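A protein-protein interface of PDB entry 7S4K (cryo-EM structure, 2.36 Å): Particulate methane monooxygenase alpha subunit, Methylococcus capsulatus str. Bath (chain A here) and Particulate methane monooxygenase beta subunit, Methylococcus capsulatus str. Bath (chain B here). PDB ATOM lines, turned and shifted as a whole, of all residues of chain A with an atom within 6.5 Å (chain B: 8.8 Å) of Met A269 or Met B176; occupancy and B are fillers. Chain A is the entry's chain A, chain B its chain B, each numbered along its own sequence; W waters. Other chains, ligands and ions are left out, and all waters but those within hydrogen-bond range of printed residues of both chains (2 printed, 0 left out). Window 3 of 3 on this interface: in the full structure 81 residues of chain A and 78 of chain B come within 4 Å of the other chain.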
ATOM      1  N   ASP A  85      -4.632  -6.173 -13.616  1.00  0.00           N
ATOM      2  CA  ASP A  85      -3.725  -6.170 -14.755  1.00  0.00           C
ATOM      3  C   ASP A  85      -4.420  -5.672 -16.010  1.00  0.00           C
ATOM      4  O   ASP A  85      -3.773  -5.101 -16.893  1.00  0.00           O
ATOM      5  CB  ASP A  85      -3.162  -7.570 -14.985  1.00  0.00           C
ATOM      6  CG  ASP A  85      -2.200  -7.996 -13.897  1.00  0.00           C
ATOM      7  OD1 ASP A  85      -1.814  -7.143 -13.073  1.00  0.00           O
ATOM      8  OD2 ASP A  85      -1.829  -9.187 -13.867  1.00  0.00           O
ATOM      9  N   GLN A 108      -3.822  11.049 -19.445  1.00  0.00           N
ATOM     10  CA  GLN A 108      -3.880  10.590 -20.822  1.00  0.00           C
ATOM     11  C   GLN A 108      -5.159   9.798 -21.073  1.00  0.00           C
ATOM     12  O   GLN A 108      -5.675   9.128 -20.174  1.00  0.00           O
ATOM     13  CB  GLN A 108      -2.648   9.749 -21.160  1.00  0.00           C
ATOM     14  CG  GLN A 108      -2.760   8.281 -20.845  1.00  0.00           C
ATOM     15  CD  GLN A 108      -1.938   7.447 -21.800  1.00  0.00           C
ATOM     16  OE1 GLN A 108      -2.336   7.220 -22.939  1.00  0.00           O
ATOM     17  NE2 GLN A 108      -0.781   6.986 -21.340  1.00  0.00           N
ATOM     18  N   LEU A 109      -5.666   9.894 -22.300  1.00  0.00           N
ATOM     19  CA  LEU A 109      -6.945   9.288 -22.646  1.00  0.00           C
ATOM     20  C   LEU A 109      -6.856   7.769 -22.615  1.00  0.00           C
ATOM     21  O   LEU A 109      -5.856   7.180 -23.031  1.00  0.00           O
ATOM     22  CB  LEU A 109      -7.388   9.765 -24.028  1.00  0.00           C
ATOM     23  CG  LEU A 109      -8.794   9.385 -24.484  1.00  0.00           C
ATOM     24  CD1 LEU A 109      -9.752  10.530 -24.228  1.00  0.00           C
ATOM     25  CD2 LEU A 109      -8.790   9.017 -25.954  1.00  0.00           C
ATOM     26  N   VAL A 110      -7.916   7.132 -22.129  1.00  0.00           N
ATOM     27  CA  VAL A 110      -7.922   5.681 -21.966  1.00  0.00           C
ATOM     28  C   VAL A 110      -9.172   5.078 -22.599  1.00  0.00           C
ATOM     29  O   VAL A 110     -10.053   4.580 -21.883  1.00  0.00           O
ATOM     30  CB  VAL A 110      -7.794   5.297 -20.481  1.00  0.00           C
ATOM     31  CG1 VAL A 110      -6.377   5.543 -20.007  1.00  0.00           C
ATOM     32  CG2 VAL A 110      -8.761   6.099 -19.625  1.00  0.00           C
ATOM     33  N   PRO A 111      -9.291   5.079 -23.930  1.00  0.00           N
ATOM     34  CA  PRO A 111     -10.449   4.429 -24.556  1.00  0.00           C
ATOM     35  C   PRO A 111     -10.435   2.920 -24.436  1.00  0.00           C
ATOM     36  O   PRO A 111     -11.492   2.294 -24.590  1.00  0.00           O
ATOM     37  CB  PRO A 111     -10.347   4.868 -26.020  1.00  0.00           C
ATOM     38  CG  PRO A 111      -8.902   5.079 -26.232  1.00  0.00           C
ATOM     39  CD  PRO A 111      -8.337   5.580 -24.932  1.00  0.00           C
ATOM     40  N   ARG A 112      -9.287   2.318 -24.164  1.00  0.00           N
ATOM     41  CA  ARG A 112      -9.155   0.880 -24.011  1.00  0.00           C
ATOM     42  C   ARG A 112      -8.949   0.533 -22.544  1.00  0.00           C
ATOM     43  O   ARG A 112      -8.904   1.401 -21.670  1.00  0.00           O
ATOM     44  CB  ARG A 112      -8.002   0.351 -24.863  1.00  0.00           C
ATOM     45  CG  ARG A 112      -7.531   1.302 -25.944  1.00  0.00           C
ATOM     46  CD  ARG A 112      -7.442   0.575 -27.271  1.00  0.00           C
ATOM     47  NE  ARG A 112      -6.571   1.246 -28.225  1.00  0.00           N
ATOM     48  CZ  ARG A 112      -5.332   0.867 -28.499  1.00  0.00           C
ATOM     49  NH1 ARG A 112      -4.770  -0.158 -27.879  1.00  0.00           N
ATOM     50  NH2 ARG A 112      -4.639   1.529 -29.419  1.00  0.00           N
ATOM     51  N   SER A 113      -8.830  -0.762 -22.279  1.00  0.00           N
ATOM     52  CA  SER A 113      -8.523  -1.221 -20.936  1.00  0.00           C
ATOM     53  C   SER A 113      -7.095  -0.841 -20.567  1.00  0.00           C
ATOM     54  O   SER A 113      -6.230  -0.670 -21.428  1.00  0.00           O
ATOM     55  CB  SER A 113      -8.712  -2.731 -20.832  1.00  0.00           C
ATOM     56  OG  SER A 113      -8.051  -3.397 -21.890  1.00  0.00           O
ATOM     57  N   VAL A 114      -6.856  -0.698 -19.268  1.00  0.00           N
ATOM     58  CA  VAL A 114      -5.567  -0.252 -18.763  1.00  0.00           C
ATOM     59  C   VAL A 114      -5.075  -1.236 -17.714  1.00  0.00           C
ATOM     60  O   VAL A 114      -5.831  -2.049 -17.178  1.00  0.00           O
ATOM     61  CB  VAL A 114      -5.632   1.171 -18.178  1.00  0.00           C
ATOM     62  CG1 VAL A 114      -6.178   2.128 -19.203  1.00  0.00           C
ATOM     63  CG2 VAL A 114      -6.489   1.188 -16.930  1.00  0.00           C
ATOM     64  N   ARG A 115      -3.782  -1.155 -17.431  1.00  0.00           N
ATOM     65  CA  ARG A 115      -3.158  -1.944 -16.380  1.00  0.00           C
ATOM     66  C   ARG A 115      -2.910  -1.054 -15.172  1.00  0.00           C
ATOM     67  O   ARG A 115      -2.267  -0.007 -15.288  1.00  0.00           O
ATOM     68  CB  ARG A 115      -1.846  -2.562 -16.859  1.00  0.00           C
ATOM     69  CG  ARG A 115      -0.970  -3.066 -15.733  1.00  0.00           C
ATOM     70  CD  ARG A 115       0.280  -3.735 -16.259  1.00  0.00           C
ATOM     71  NE  ARG A 115       0.111  -5.176 -16.384  1.00  0.00           N
ATOM     72  CZ  ARG A 115       0.621  -6.063 -15.543  1.00  0.00           C
ATOM     73  NH1 ARG A 115       1.340  -5.690 -14.499  1.00  0.00           N
ATOM     74  NH2 ARG A 115       0.406  -7.358 -15.756  1.00  0.00           N
ATOM     75  N   LEU A 116      -3.420  -1.473 -14.022  1.00  0.00           N
ATOM     76  CA  LEU A 116      -3.250  -0.749 -12.773  1.00  0.00           C
ATOM     77  C   LEU A 116      -2.380  -1.567 -11.833  1.00  0.00           C
ATOM     78  O   LEU A 116      -2.417  -2.801 -11.854  1.00  0.00           O
ATOM     79  CB  LEU A 116      -4.601  -0.457 -12.118  1.00  0.00           C
ATOM     80  CG  LEU A 116      -5.601   0.323 -12.970  1.00  0.00           C
ATOM     81  CD1 LEU A 116      -6.952   0.361 -12.290  1.00  0.00           C
ATOM     82  CD2 LEU A 116      -5.095   1.727 -13.240  1.00  0.00           C
ATOM     83  N   GLY A 267      -6.611  -3.227 -27.422  1.00  0.00           N
ATOM     84  CA  GLY A 267      -5.383  -3.596 -26.750  1.00  0.00           C
ATOM     85  C   GLY A 267      -5.207  -2.883 -25.428  1.00  0.00           C
ATOM     86  O   GLY A 267      -5.402  -1.669 -25.342  1.00  0.00           O
ATOM     87  N   THR A 268      -4.842  -3.631 -24.390  1.00  0.00           N
ATOM     88  CA  THR A 268      -4.644  -3.040 -23.076  1.00  0.00           C
ATOM     89  C   THR A 268      -3.502  -2.034 -23.112  1.00  0.00           C
ATOM     90  O   THR A 268      -2.446  -2.285 -23.697  1.00  0.00           O
ATOM     91  CB  THR A 268      -4.355  -4.128 -22.043  1.00  0.00           C
ATOM     92  OG1 THR A 268      -5.447  -5.054 -22.010  1.00  0.00           O
ATOM     93  CG2 THR A 268      -4.177  -3.525 -20.662  1.00  0.00           C
ATOM     94  N   MET A 269      -3.724  -0.886 -22.486  1.00  0.00           N
ATOM     95  CA  MET A 269      -2.754   0.199 -22.457  1.00  0.00           C
ATOM     96  C   MET A 269      -1.966   0.123 -21.157  1.00  0.00           C
ATOM     97  O   MET A 269      -2.531   0.289 -20.072  1.00  0.00           O
ATOM     98  CB  MET A 269      -3.463   1.544 -22.586  1.00  0.00           C
ATOM     99  CG  MET A 269      -3.939   1.847 -23.993  1.00  0.00           C
ATOM    100  SD  MET A 269      -4.781   3.431 -24.107  1.00  0.00           S
ATOM    101  CE  MET A 269      -3.676   4.447 -23.145  1.00  0.00           C
ATOM    102  N   ARG A 270      -0.666  -0.125 -21.268  1.00  0.00           N
ATOM    103  CA  ARG A 270       0.222  -0.176 -20.119  1.00  0.00           C
ATOM    104  C   ARG A 270       0.748   1.223 -19.815  1.00  0.00           C
ATOM    105  O   ARG A 270       0.444   2.197 -20.505  1.00  0.00           O
ATOM    106  CB  ARG A 270       1.375  -1.146 -20.375  1.00  0.00           C
ATOM    107  CG  ARG A 270       1.256  -2.474 -19.660  1.00  0.00           C
ATOM    108  CD  ARG A 270       2.182  -3.500 -20.290  1.00  0.00           C
ATOM    109  NE  ARG A 270       2.371  -4.677 -19.452  1.00  0.00           N
ATOM    110  CZ  ARG A 270       3.123  -4.709 -18.361  1.00  0.00           C
ATOM    111  NH1 ARG A 270       3.776  -3.639 -17.940  1.00  0.00           N
ATOM    112  NH2 ARG A 270       3.225  -5.844 -17.679  1.00  0.00           N
ATOM    113  N   GLY A 271       1.558   1.316 -18.767  1.00  0.00           N
ATOM    114  CA  GLY A 271       2.196   2.569 -18.419  1.00  0.00           C
ATOM    115  C   GLY A 271       1.250   3.666 -17.981  1.00  0.00           C
ATOM    116  O   GLY A 271       1.382   4.814 -18.413  1.00  0.00           O
ATOM    117  N   MET A 272       0.287   3.330 -17.128  1.00  0.00           N
ATOM    118  CA  MET A 272      -0.581   4.333 -16.521  1.00  0.00           C
ATOM    119  C   MET A 272       0.221   5.071 -15.459  1.00  0.00           C
ATOM    120  O   MET A 272       0.765   4.451 -14.542  1.00  0.00           O
ATOM    121  CB  MET A 272      -1.820   3.680 -15.918  1.00  0.00           C
ATOM    122  CG  MET A 272      -2.864   3.254 -16.932  1.00  0.00           C
ATOM    123  SD  MET A 272      -3.363   4.589 -18.031  1.00  0.00           S
ATOM    124  CE  MET A 272      -2.652   4.030 -19.574  1.00  0.00           C
ATOM    125  N   PRO B 170     -11.158   5.549 -40.346  1.00  0.00           N
ATOM    126  CA  PRO B 170     -10.304   5.999 -39.243  1.00  0.00           C
ATOM    127  C   PRO B 170     -10.694   7.387 -38.764  1.00  0.00           C
ATOM    128  O   PRO B 170     -11.105   8.245 -39.545  1.00  0.00           O
ATOM    129  CB  PRO B 170      -8.901   5.993 -39.855  1.00  0.00           C
ATOM    130  CG  PRO B 170      -9.130   6.134 -41.309  1.00  0.00           C
ATOM    131  CD  PRO B 170     -10.409   5.420 -41.605  1.00  0.00           C
ATOM    132  N   VAL B 171     -10.562   7.599 -37.459  1.00  0.00           N
ATOM    133  CA  VAL B 171     -10.822   8.892 -36.841  1.00  0.00           C
ATOM    134  C   VAL B 171      -9.719   9.178 -35.836  1.00  0.00           C
ATOM    135  O   VAL B 171      -9.307   8.292 -35.081  1.00  0.00           O
ATOM    136  CB  VAL B 171     -12.202   8.940 -36.150  1.00  0.00           C
ATOM    137  CG1 VAL B 171     -12.419  10.291 -35.497  1.00  0.00           C
ATOM    138  CG2 VAL B 171     -13.316   8.645 -37.132  1.00  0.00           C
ATOM    139  N   GLU B 172      -9.232  10.414 -35.839  1.00  0.00           N
ATOM    140  CA  GLU B 172      -8.344  10.904 -34.790  1.00  0.00           C
ATOM    141  C   GLU B 172      -9.211  11.367 -33.631  1.00  0.00           C
ATOM    142  O   GLU B 172      -9.824  12.434 -33.686  1.00  0.00           O
ATOM    143  CB  GLU B 172      -7.468  12.034 -35.311  1.00  0.00           C
ATOM    144  CG  GLU B 172      -6.040  11.990 -34.828  1.00  0.00           C
ATOM    145  CD  GLU B 172      -5.829  12.781 -33.559  1.00  0.00           C
ATOM    146  OE1 GLU B 172      -6.811  13.343 -33.030  1.00  0.00           O
ATOM    147  OE2 GLU B 172      -4.672  12.855 -33.098  1.00  0.00           O
ATOM    148  N   TYR B 173      -9.273  10.564 -32.579  1.00  0.00           N
ATOM    149  CA  TYR B 173     -10.144  10.834 -31.439  1.00  0.00           C
ATOM    150  C   TYR B 173      -9.272  11.166 -30.236  1.00  0.00           C
ATOM    151  O   TYR B 173      -8.775  10.263 -29.556  1.00  0.00           O
ATOM    152  CB  TYR B 173     -11.057   9.648 -31.161  1.00  0.00           C
ATOM    153  CG  TYR B 173     -12.249   9.994 -30.306  1.00  0.00           C
ATOM    154  CD1 TYR B 173     -13.373  10.585 -30.860  1.00  0.00           C
ATOM    155  CD2 TYR B 173     -12.253   9.725 -28.947  1.00  0.00           C
ATOM    156  CE1 TYR B 173     -14.463  10.903 -30.085  1.00  0.00           C
ATOM    157  CE2 TYR B 173     -13.340  10.038 -28.164  1.00  0.00           C
ATOM    158  CZ  TYR B 173     -14.441  10.627 -28.739  1.00  0.00           C
ATOM    159  OH  TYR B 173     -15.529  10.942 -27.963  1.00  0.00           O
ATOM    160  N   ASN B 174      -9.098  12.461 -29.980  1.00  0.00           N
ATOM    161  CA  ASN B 174      -8.341  12.949 -28.828  1.00  0.00           C
ATOM    162  C   ASN B 174      -6.925  12.380 -28.807  1.00  0.00           C
ATOM    163  O   ASN B 174      -6.408  11.976 -27.764  1.00  0.00           O
ATOM    164  CB  ASN B 174      -9.073  12.639 -27.523  1.00  0.00           C
ATOM    165  CG  ASN B 174     -10.406  13.348 -27.424  1.00  0.00           C
ATOM    166  OD1 ASN B 174     -11.461  12.715 -27.423  1.00  0.00           O
ATOM    167  ND2 ASN B 174     -10.366  14.671 -27.339  1.00  0.00           N
ATOM    168  N   GLY B 175      -6.290  12.347 -29.975  1.00  0.00           N
ATOM    169  CA  GLY B 175      -4.912  11.929 -30.085  1.00  0.00           C
ATOM    170  C   GLY B 175      -4.695  10.454 -30.333  1.00  0.00           C
ATOM    171  O   GLY B 175      -3.553  10.050 -30.578  1.00  0.00           O
ATOM    172  N   MET B 176      -5.740   9.638 -30.280  1.00  0.00           N
ATOM    173  CA  MET B 176      -5.629   8.207 -30.509  1.00  0.00           C
ATOM    174  C   MET B 176      -6.399   7.830 -31.764  1.00  0.00           C
ATOM    175  O   MET B 176      -7.471   8.378 -32.033  1.00  0.00           O
ATOM    176  CB  MET B 176      -6.161   7.415 -29.312  1.00  0.00           C
ATOM    177  CG  MET B 176      -5.190   7.339 -28.148  1.00  0.00           C
ATOM    178  SD  MET B 176      -5.467   5.914 -27.086  1.00  0.00           S
ATOM    179  CE  MET B 176      -4.726   4.615 -28.066  1.00  0.00           C
ATOM    180  N   LEU B 177      -5.845   6.904 -32.537  1.00  0.00           N
ATOM    181  CA  LEU B 177      -6.523   6.433 -33.736  1.00  0.00           C
ATOM    182  C   LEU B 177      -7.637   5.481 -33.335  1.00  0.00           C
ATOM    183  O   LEU B 177      -7.402   4.508 -32.613  1.00  0.00           O
ATOM    184  CB  LEU B 177      -5.550   5.745 -34.686  1.00  0.00           C
ATOM    185  CG  LEU B 177      -6.265   5.147 -35.896  1.00  0.00           C
ATOM    186  CD1 LEU B 177      -6.797   6.253 -36.774  1.00  0.00           C
ATOM    187  CD2 LEU B 177      -5.361   4.233 -36.687  1.00  0.00           C
ATOM    188  N   MET B 178      -8.851   5.772 -33.785  1.00  0.00           N
ATOM    189  CA  MET B 178      -9.998   4.921 -33.525  1.00  0.00           C
ATOM    190  C   MET B 178     -10.848   4.845 -34.781  1.00  0.00           C
ATOM    191  O   MET B 178     -10.970   5.819 -35.525  1.00  0.00           O
ATOM    192  CB  MET B 178     -10.843   5.442 -32.355  1.00  0.00           C
ATOM    193  CG  MET B 178     -10.084   5.599 -31.048  1.00  0.00           C
ATOM    194  SD  MET B 178     -11.087   6.282 -29.721  1.00  0.00           S
ATOM    195  CE  MET B 178     -12.119   4.879 -29.324  1.00  0.00           C
ATOM    196  N   SER B 179     -11.424   3.675 -35.016  1.00  0.00           N
ATOM    197  CA  SER B 179     -12.452   3.563 -36.030  1.00  0.00           C
ATOM    198  C   SER B 179     -13.764   4.127 -35.495  1.00  0.00           C
ATOM    199  O   SER B 179     -13.916   4.391 -34.301  1.00  0.00           O
ATOM    200  CB  SER B 179     -12.613   2.111 -36.470  1.00  0.00           C
ATOM    201  OG  SER B 179     -13.080   1.307 -35.406  1.00  0.00           O
ATOM    202  N   ASP B 182     -15.177   1.890 -32.899  1.00  0.00           N
ATOM    203  CA  ASP B 182     -14.504   2.063 -31.616  1.00  0.00           C
ATOM    204  C   ASP B 182     -15.041   3.280 -30.880  1.00  0.00           C
ATOM    205  O   ASP B 182     -15.245   3.238 -29.664  1.00  0.00           O
ATOM    206  CB  ASP B 182     -12.997   2.192 -31.823  1.00  0.00           C
ATOM    207  CG  ASP B 182     -12.342   0.877 -32.165  1.00  0.00           C
ATOM    208  OD1 ASP B 182     -12.695  -0.146 -31.544  1.00  0.00           O
ATOM    209  OD2 ASP B 182     -11.468   0.865 -33.054  1.00  0.00           O
ATOM    210  N   ILE B 183     -15.275   4.375 -31.603  1.00  0.00           N
ATOM    211  CA  ILE B 183     -15.815   5.574 -30.974  1.00  0.00           C
ATOM    212  C   ILE B 183     -17.236   5.332 -30.492  1.00  0.00           C
ATOM    213  O   ILE B 183     -17.640   5.843 -29.445  1.00  0.00           O
ATOM    214  CB  ILE B 183     -15.739   6.765 -31.941  1.00  0.00           C
ATOM    215  CG1 ILE B 183     -14.286   7.096 -32.244  1.00  0.00           C
ATOM    216  CG2 ILE B 183     -16.420   7.978 -31.354  1.00  0.00           C
ATOM    217  CD1 ILE B 183     -14.139   7.998 -33.402  1.00  0.00           C
ATOM    218  N   TYR B 186     -16.928   3.448 -27.316  1.00  0.00           N
ATOM    219  CA  TYR B 186     -16.412   4.316 -26.265  1.00  0.00           C
ATOM    220  C   TYR B 186     -17.482   5.275 -25.757  1.00  0.00           C
ATOM    221  O   TYR B 186     -17.655   5.433 -24.544  1.00  0.00           O
ATOM    222  CB  TYR B 186     -15.201   5.083 -26.791  1.00  0.00           C
ATOM    223  CG  TYR B 186     -14.474   5.890 -25.750  1.00  0.00           C
ATOM    224  CD1 TYR B 186     -14.086   5.318 -24.549  1.00  0.00           C
ATOM    225  CD2 TYR B 186     -14.166   7.221 -25.972  1.00  0.00           C
ATOM    226  CE1 TYR B 186     -13.419   6.052 -23.598  1.00  0.00           C
ATOM    227  CE2 TYR B 186     -13.499   7.963 -25.029  1.00  0.00           C
ATOM    228  CZ  TYR B 186     -13.127   7.372 -23.844  1.00  0.00           C
ATOM    229  OH  TYR B 186     -12.459   8.109 -22.898  1.00  0.00           O
ATOM    230  N   GLU B 195     -14.535  -2.558 -21.862  1.00  0.00           N
ATOM    231  CA  GLU B 195     -13.799  -2.732 -23.108  1.00  0.00           C
ATOM    232  C   GLU B 195     -13.039  -4.050 -23.135  1.00  0.00           C
ATOM    233  O   GLU B 195     -12.997  -4.712 -24.175  1.00  0.00           O
ATOM    234  CB  GLU B 195     -12.864  -1.536 -23.323  1.00  0.00           C
ATOM    235  CG  GLU B 195     -12.251  -1.384 -24.723  1.00  0.00           C
ATOM    236  CD  GLU B 195     -10.962  -2.161 -24.962  1.00  0.00           C
ATOM    237  OE1 GLU B 195     -10.708  -3.184 -24.304  1.00  0.00           O
ATOM    238  OE2 GLU B 195     -10.190  -1.743 -25.849  1.00  0.00           O
ATOM    239  N   LYS B 202      -6.556  -8.524 -31.692  1.00  0.00           N
ATOM    240  CA  LYS B 202      -5.628  -7.635 -31.017  1.00  0.00           C
ATOM    241  C   LYS B 202      -4.204  -7.746 -31.536  1.00  0.00           C
ATOM    242  O   LYS B 202      -3.322  -7.056 -31.015  1.00  0.00           O
ATOM    243  CB  LYS B 202      -5.630  -7.909 -29.507  1.00  0.00           C
ATOM    244  CG  LYS B 202      -6.465  -6.946 -28.694  1.00  0.00           C
ATOM    245  CD  LYS B 202      -7.165  -7.668 -27.562  1.00  0.00           C
ATOM    246  CE  LYS B 202      -8.191  -6.777 -26.891  1.00  0.00           C
ATOM    247  NZ  LYS B 202      -9.155  -7.564 -26.075  1.00  0.00           N
HETATM  248  O   HOH W   1      -8.014   3.223 -29.468  1.00  0.00           O
HETATM  249  O   HOH W   2      -5.277   3.038 -31.968  1.00  0.00           O
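NH1 of Arg A112 sits at hydrogen-bond distance from O of Gly A267, 3.0 Å away.
The side-chain hydroxyl (OG1) of Thr A268 sits at hydrogen-bond distance from the side-chain hydroxyl (OG) of Ser A113 (3.1 Å).
The backbone carbonyl oxygen (O) of Ser A113 is in hydrogen-bond range of the backbone NH (N) of Met A269 (2.7 Å).
The backbone carbonyl oxygen (O) of Met A269 is in hydrogen-bond range of the backbone NH (N) of Arg A115, at 3.3 Å.
The backbone carbonyl oxygen of Met B178 sits at hydrogen-bond distance from the backbone NH of Val B171 (2.7 Å).
Among the printed residues, merely in contact across the chains: Arg A112 with Glu B195 (3.2 Å), Arg A112 with Met B176 (3.4 Å), Pro A111 with Tyr B186 (3.5 Å), Ser A113 with Glu B195 (3.6 Å), Pro A111 with Met B176 (3.6 Å), Pro A111 with Met B178 (3.7 Å), Pro A111 with Glu B195 (3.8 Å), Leu A109 with Tyr B173 (3.8 Å), Leu A109 with Tyr B186 (3.9 Å), Gly A267 with Lys B202 (3.9 Å), Met A269 with Met B176 (3.9 Å) and Leu A109 with Asn B174 (3.96 Å).
Of the printed residues of chain B, Met A269 touches Met B176.
Of chain A, only Pro A111 (3.6 Å), Arg A112 (3.4 Å) and Met A269 (3.9 Å) come within 4 Å of Met B176.
No residue of chain B comes within 4 Å of Thr A268.
Printed residues of chain A within 4 Å of Tyr B173: Leu A109.
Of the printed residues of chain A, Met B178 touches Pro A111 (3.7 Å).
Printed residues of chain B within 4 Å of Gly A267: Lys B202.
Printed residues of chain A within 4 Å of Tyr B186: Leu A109 and Pro A111.
Printed residues of chain A within 4 Å of Asn B174: Leu A109.
The nearest residue of chain B that does not touch Met A269 is Glu B195 (7.3 Å).
The nearest printed residue of chain A that does not touch Glu B195 is Gly A267 (4.2 Å).
Of the 16 printed residues of chain A, 6 touch a printed residue of chain B.
Hydrophobic or aromatic side chains of chain A that line the printed part of chain B: Leu A109, Pro A111 and Met A269.
Of the 15 printed residues of chain B, 7 touch a printed residue of chain A.
Among the printed residues, 12 pairs touch across the chains.
Among the printed residues, no Asp or Glu carboxylate lies within 4 Å of a Lys or Arg side-chain nitrogen of the other chain.
Water W2 bridges the backbone carbonyl oxygen (O) of Leu B177 and the guanidinium group (NH2) of Arg A112.
Water W1 lies within hydrogen-bond range of the guanidinium group of Arg A112 (2.7 Å) and the backbone carbonyl oxygen of Leu B177 (3.5 Å).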
